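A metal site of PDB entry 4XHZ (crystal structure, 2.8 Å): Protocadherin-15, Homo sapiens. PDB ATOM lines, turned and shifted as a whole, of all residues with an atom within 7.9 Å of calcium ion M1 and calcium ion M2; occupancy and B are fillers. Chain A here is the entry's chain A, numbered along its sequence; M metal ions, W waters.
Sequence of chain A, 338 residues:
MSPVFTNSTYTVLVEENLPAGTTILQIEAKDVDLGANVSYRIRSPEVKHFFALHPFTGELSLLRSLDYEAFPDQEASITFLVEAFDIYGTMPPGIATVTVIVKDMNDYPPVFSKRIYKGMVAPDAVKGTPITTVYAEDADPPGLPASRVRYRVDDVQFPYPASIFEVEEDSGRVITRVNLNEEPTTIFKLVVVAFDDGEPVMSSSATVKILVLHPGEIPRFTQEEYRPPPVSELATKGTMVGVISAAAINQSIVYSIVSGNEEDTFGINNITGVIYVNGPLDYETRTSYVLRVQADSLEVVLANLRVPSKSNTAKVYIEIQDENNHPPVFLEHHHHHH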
ATOM      1  N   GLU A  16       7.238  -6.170 -14.263  1.00  0.00           N
ATOM      2  CA  GLU A  16       7.560  -5.004 -15.083  1.00  0.00           C
ATOM      3  C   GLU A  16       6.681  -4.994 -16.319  1.00  0.00           C
ATOM      4  O   GLU A  16       6.212  -6.033 -16.764  1.00  0.00           O
ATOM      5  CB  GLU A  16       9.045  -4.971 -15.459  1.00  0.00           C
ATOM      6  CG  GLU A  16       9.524  -6.050 -16.425  1.00  0.00           C
ATOM      7  CD  GLU A  16      10.867  -5.685 -17.063  1.00  0.00           C
ATOM      8  OE1 GLU A  16      11.002  -4.542 -17.548  1.00  0.00           O
ATOM      9  OE2 GLU A  16      11.779  -6.531 -17.070  1.00  0.00           O
ATOM     10  N   ASN A  17       6.439  -3.805 -16.868  1.00  0.00           N
ATOM     11  CA  ASN A  17       5.678  -3.688 -18.115  1.00  0.00           C
ATOM     12  C   ASN A  17       4.192  -3.975 -17.979  1.00  0.00           C
ATOM     13  O   ASN A  17       3.555  -4.297 -18.968  1.00  0.00           O
ATOM     14  CB  ASN A  17       6.263  -4.599 -19.204  1.00  0.00           C
ATOM     15  CG  ASN A  17       7.711  -4.269 -19.538  1.00  0.00           C
ATOM     16  OD1 ASN A  17       8.124  -3.100 -19.515  1.00  0.00           O
ATOM     17  ND2 ASN A  17       8.496  -5.299 -19.848  1.00  0.00           N
ATOM     18  N   LEU A  66       6.365  -0.188 -14.841  1.00  0.00           N
ATOM     19  CA  LEU A  66       7.699  -0.356 -14.279  1.00  0.00           C
ATOM     20  C   LEU A  66       8.638  -0.985 -15.287  1.00  0.00           C
ATOM     21  O   LEU A  66       8.198  -1.709 -16.190  1.00  0.00           O
ATOM     22  CB  LEU A  66       7.633  -1.193 -13.015  1.00  0.00           C
ATOM     23  CG  LEU A  66       6.833  -0.498 -11.920  1.00  0.00           C
ATOM     24  CD1 LEU A  66       6.619  -1.418 -10.721  1.00  0.00           C
ATOM     25  CD2 LEU A  66       7.554   0.764 -11.501  1.00  0.00           C
ATOM     26  N   ASP A  67       9.936  -0.718 -15.129  1.00  0.00           N
ATOM     27  CA  ASP A  67      10.976  -1.327 -15.977  1.00  0.00           C
ATOM     28  C   ASP A  67      12.126  -1.918 -15.132  1.00  0.00           C
ATOM     29  O   ASP A  67      12.974  -1.180 -14.597  1.00  0.00           O
ATOM     30  CB  ASP A  67      11.501  -0.286 -16.977  1.00  0.00           C
ATOM     31  CG  ASP A  67      12.728  -0.764 -17.741  1.00  0.00           C
ATOM     32  OD1 ASP A  67      13.091  -1.960 -17.655  1.00  0.00           O
ATOM     33  OD2 ASP A  67      13.323   0.074 -18.444  1.00  0.00           O
ATOM     34  N   TYR A  68      12.164  -3.237 -15.035  1.00  0.00           N
ATOM     35  CA  TYR A  68      13.191  -3.911 -14.250  1.00  0.00           C
ATOM     36  C   TYR A  68      14.605  -3.381 -14.529  1.00  0.00           C
ATOM     37  O   TYR A  68      15.389  -3.076 -13.617  1.00  0.00           O
ATOM     38  CB  TYR A  68      13.150  -5.423 -14.500  1.00  0.00           C
ATOM     39  CG  TYR A  68      14.151  -6.157 -13.656  1.00  0.00           C
ATOM     40  CD1 TYR A  68      15.488  -6.255 -14.054  1.00  0.00           C
ATOM     41  CD2 TYR A  68      13.787  -6.726 -12.449  1.00  0.00           C
ATOM     42  CE1 TYR A  68      16.414  -6.907 -13.266  1.00  0.00           C
ATOM     43  CE2 TYR A  68      14.703  -7.384 -11.669  1.00  0.00           C
ATOM     44  CZ  TYR A  68      16.016  -7.458 -12.072  1.00  0.00           C
ATOM     45  OH  TYR A  68      16.936  -8.102 -11.293  1.00  0.00           O
ATOM     46  N   GLU A  69      14.940  -3.301 -15.809  1.00  0.00           N
ATOM     47  CA  GLU A  69      16.278  -2.934 -16.240  1.00  0.00           C
ATOM     48  C   GLU A  69      16.636  -1.472 -15.943  1.00  0.00           C
ATOM     49  O   GLU A  69      17.788  -1.074 -16.031  1.00  0.00           O
ATOM     50  CB  GLU A  69      16.464  -3.242 -17.741  1.00  0.00           C
ATOM     51  CG  GLU A  69      16.776  -4.700 -18.068  1.00  0.00           C
ATOM     52  CD  GLU A  69      15.547  -5.599 -18.041  1.00  0.00           C
ATOM     53  OE1 GLU A  69      14.444  -5.108 -18.359  1.00  0.00           O
ATOM     54  OE2 GLU A  69      15.695  -6.802 -17.707  1.00  0.00           O
ATOM     55  N   ALA A  70      15.651  -0.666 -15.588  1.00  0.00           N
ATOM     56  CA  ALA A  70      15.879   0.747 -15.402  1.00  0.00           C
ATOM     57  C   ALA A  70      16.414   1.045 -14.017  1.00  0.00           C
ATOM     58  O   ALA A  70      16.810   2.184 -13.722  1.00  0.00           O
ATOM     59  CB  ALA A  70      14.607   1.532 -15.666  1.00  0.00           C
ATOM     60  N   LYS A 103       9.453  -7.504 -10.673  1.00  0.00           N
ATOM     61  CA  LYS A 103       9.851  -8.795 -11.242  1.00  0.00           C
ATOM     62  C   LYS A 103      10.343  -8.644 -12.665  1.00  0.00           C
ATOM     63  O   LYS A 103       9.665  -8.019 -13.504  1.00  0.00           O
ATOM     64  CB  LYS A 103       8.704  -9.790 -11.203  1.00  0.00           C
ATOM     65  CG  LYS A 103       9.172 -11.187 -11.560  1.00  0.00           C
ATOM     66  CD  LYS A 103       8.008 -12.149 -11.619  1.00  0.00           C
ATOM     67  CE  LYS A 103       8.520 -13.571 -11.585  1.00  0.00           C
ATOM     68  NZ  LYS A 103       7.551 -14.462 -12.251  1.00  0.00           N
ATOM     69  N   ASP A 104      11.512  -9.220 -12.948  1.00  0.00           N
ATOM     70  CA  ASP A 104      12.058  -9.195 -14.299  1.00  0.00           C
ATOM     71  C   ASP A 104      11.192 -10.001 -15.291  1.00  0.00           C
ATOM     72  O   ASP A 104      10.667 -11.074 -14.959  1.00  0.00           O
ATOM     73  CB  ASP A 104      13.511  -9.703 -14.282  1.00  0.00           C
ATOM     74  CG  ASP A 104      14.216  -9.498 -15.615  1.00  0.00           C
ATOM     75  OD1 ASP A 104      13.651  -8.871 -16.543  1.00  0.00           O
ATOM     76  OD2 ASP A 104      15.360  -9.956 -15.740  1.00  0.00           O
ATOM     77  N   MET A 105      11.008  -9.477 -16.505  1.00  0.00           N
ATOM     78  CA  MET A 105      10.218 -10.171 -17.529  1.00  0.00           C
ATOM     79  C   MET A 105      10.924 -10.118 -18.868  1.00  0.00           C
ATOM     80  O   MET A 105      11.876  -9.350 -19.061  1.00  0.00           O
ATOM     81  CB  MET A 105       8.827  -9.547 -17.667  1.00  0.00           C
ATOM     82  CG  MET A 105       8.013  -9.576 -16.395  1.00  0.00           C
ATOM     83  SD  MET A 105       7.006 -11.059 -16.212  1.00  0.00           S
ATOM     84  CE  MET A 105       7.968 -12.055 -15.073  1.00  0.00           C
ATOM     85  N   ASN A 106      10.465 -10.936 -19.795  1.00  0.00           N
ATOM     86  CA  ASN A 106      11.043 -10.942 -21.122  1.00  0.00           C
ATOM     87  C   ASN A 106      10.640  -9.633 -21.860  1.00  0.00           C
ATOM     88  O   ASN A 106       9.452  -9.319 -21.947  1.00  0.00           O
ATOM     89  CB  ASN A 106      10.619 -12.233 -21.850  1.00  0.00           C
ATOM     90  CG  ASN A 106      10.878 -12.202 -23.336  1.00  0.00           C
ATOM     91  OD1 ASN A 106      12.021 -12.041 -23.796  1.00  0.00           O
ATOM     92  ND2 ASN A 106       9.816 -12.400 -24.120  1.00  0.00           N
ATOM     93  N   ASP A 107      11.619  -8.871 -22.357  1.00  0.00           N
ATOM     94  CA  ASP A 107      11.336  -7.563 -22.981  1.00  0.00           C
ATOM     95  C   ASP A 107      11.190  -7.556 -24.501  1.00  0.00           C
ATOM     96  O   ASP A 107      10.299  -6.896 -25.051  1.00  0.00           O
ATOM     97  CB  ASP A 107      12.372  -6.522 -22.573  1.00  0.00           C
ATOM     98  CG  ASP A 107      12.187  -6.052 -21.169  1.00  0.00           C
ATOM     99  OD1 ASP A 107      12.313  -6.884 -20.251  1.00  0.00           O
ATOM    100  OD2 ASP A 107      11.899  -4.858 -20.964  1.00  0.00           O
ATOM    101  N   TYR A 108      12.069  -8.271 -25.193  1.00  0.00           N
ATOM    102  CA  TYR A 108      12.128  -8.178 -26.642  1.00  0.00           C
ATOM    103  C   TYR A 108      11.843  -9.474 -27.362  1.00  0.00           C
ATOM    104  O   TYR A 108      12.175 -10.565 -26.859  1.00  0.00           O
ATOM    105  CB  TYR A 108      13.490  -7.669 -27.072  1.00  0.00           C
ATOM    106  CG  TYR A 108      14.014  -6.539 -26.252  1.00  0.00           C
ATOM    107  CD1 TYR A 108      13.487  -5.259 -26.382  1.00  0.00           C
ATOM    108  CD2 TYR A 108      15.046  -6.739 -25.336  1.00  0.00           C
ATOM    109  CE1 TYR A 108      13.985  -4.212 -25.635  1.00  0.00           C
ATOM    110  CE2 TYR A 108      15.535  -5.696 -24.587  1.00  0.00           C
ATOM    111  CZ  TYR A 108      15.002  -4.438 -24.736  1.00  0.00           C
ATOM    112  OH  TYR A 108      15.495  -3.404 -23.988  1.00  0.00           O
ATOM    113  N   ASP A 140      17.391  -9.650 -25.189  1.00  0.00           N
ATOM    114  CA  ASP A 140      17.356  -9.917 -23.741  1.00  0.00           C
ATOM    115  C   ASP A 140      18.683 -10.512 -23.228  1.00  0.00           C
ATOM    116  O   ASP A 140      19.452 -11.083 -24.000  1.00  0.00           O
ATOM    117  CB  ASP A 140      16.201 -10.843 -23.392  1.00  0.00           C
ATOM    118  CG  ASP A 140      14.838 -10.173 -23.558  1.00  0.00           C
ATOM    119  OD1 ASP A 140      14.424  -9.434 -22.641  1.00  0.00           O
ATOM    120  OD2 ASP A 140      14.196 -10.393 -24.600  1.00  0.00           O
ATOM    121  N   PRO A 141      18.941 -10.364 -21.915  1.00  0.00           N
ATOM    122  CA  PRO A 141      20.117 -10.940 -21.252  1.00  0.00           C
ATOM    123  C   PRO A 141      20.507 -12.298 -21.838  1.00  0.00           C
ATOM    124  O   PRO A 141      19.697 -13.229 -21.831  1.00  0.00           O
ATOM    125  CB  PRO A 141      19.638 -11.121 -19.790  1.00  0.00           C
ATOM    126  CG  PRO A 141      18.210 -10.607 -19.741  1.00  0.00           C
ATOM    127  CD  PRO A 141      18.046  -9.724 -20.939  1.00  0.00           C
ATOM    128  N   ALA A 146      14.914 -16.448 -21.983  1.00  0.00           N
ATOM    129  CA  ALA A 146      14.238 -15.324 -22.619  1.00  0.00           C
ATOM    130  C   ALA A 146      15.001 -14.773 -23.850  1.00  0.00           C
ATOM    131  O   ALA A 146      14.462 -13.971 -24.625  1.00  0.00           O
ATOM    132  CB  ALA A 146      13.977 -14.207 -21.615  1.00  0.00           C
ATOM    133  N   GLU A 199       9.012 -15.172 -20.163  1.00  0.00           N
ATOM    134  CA  GLU A 199       7.705 -14.899 -19.601  1.00  0.00           C
ATOM    135  C   GLU A 199       7.366 -13.504 -20.110  1.00  0.00           C
ATOM    136  O   GLU A 199       8.071 -12.511 -19.712  1.00  0.00           O
ATOM    137  CB  GLU A 199       7.756 -14.990 -18.118  1.00  0.00           C
ATOM    138  CG  GLU A 199       6.756 -15.976 -17.537  1.00  0.00           C
ATOM    139  CD  GLU A 199       6.874 -16.027 -16.030  1.00  0.00           C
ATOM    140  OE1 GLU A 199       8.025 -16.008 -15.531  1.00  0.00           O
ATOM    141  OE2 GLU A 199       5.835 -16.041 -15.342  1.00  0.00           O
HETATM  142 CA    CA M   1      13.525  -7.784 -18.538  1.00  0.00          CA
HETATM  143 CA    CA M   2      12.919  -3.631 -19.321  1.00  0.00          CA
HETATM  144  O   HOH W   1      10.755  -2.679 -19.493  1.00  0.00           O
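The backbone NH of Asp 107 is in hydrogen-bond range of the side-chain carboxylate of Asp 140 (2.9 Å). The side-chain carboxylate (OE1) of Glu 16 lies close to the backbone NH (N) of Tyr 68, 3.1 Å away. OE1 of Glu 16 sits close to ND2 of Asn 17 (3.5 Å). The backbone NH (N) of Glu 16 lies within hydrogen-bond range of the backbone carbonyl oxygen (O) of Lys 103.
Within 4 Å of calcium ion M1: Glu 16, Glu 69, Asp 104, Met 105 and Asp 107. The nearest printed residue that does not touch calcium ion M1 is Asp 140 (4.5 Å).
Within 4 Å of calcium ion M2: Glu 16, Asp 67, Glu 69 and Asp 107. The nearest printed residue that does not touch calcium ion M2 is Tyr 68 (4.4 Å).
Calcium ion M1 is bound by the side-chain carboxylate (OD1) of Asp 104, the side-chain carboxylate (OD1) of Asp 107, the backbone carbonyl oxygen (O) of Met 105, the side-chain carboxylate (OE2) of Glu 69, the side-chain carboxylate (OE2) of Glu 16 and the side-chain carboxylate (OE1) of Glu 69. Calcium ion M1 has six donor atoms within binding distance.
Calcium ion M2 is bound by the side-chain carboxylate (OD2) of Asp 107 (2.3 Å), the side-chain carboxylate (OE1) of Glu 69 (2.3 Å), the side-chain carboxylate (OD1) of Asp 67 (2.4 Å), water W1 (2.4 Å) and the side-chain carboxylate (OE1) of Glu 16 (2.8 Å).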
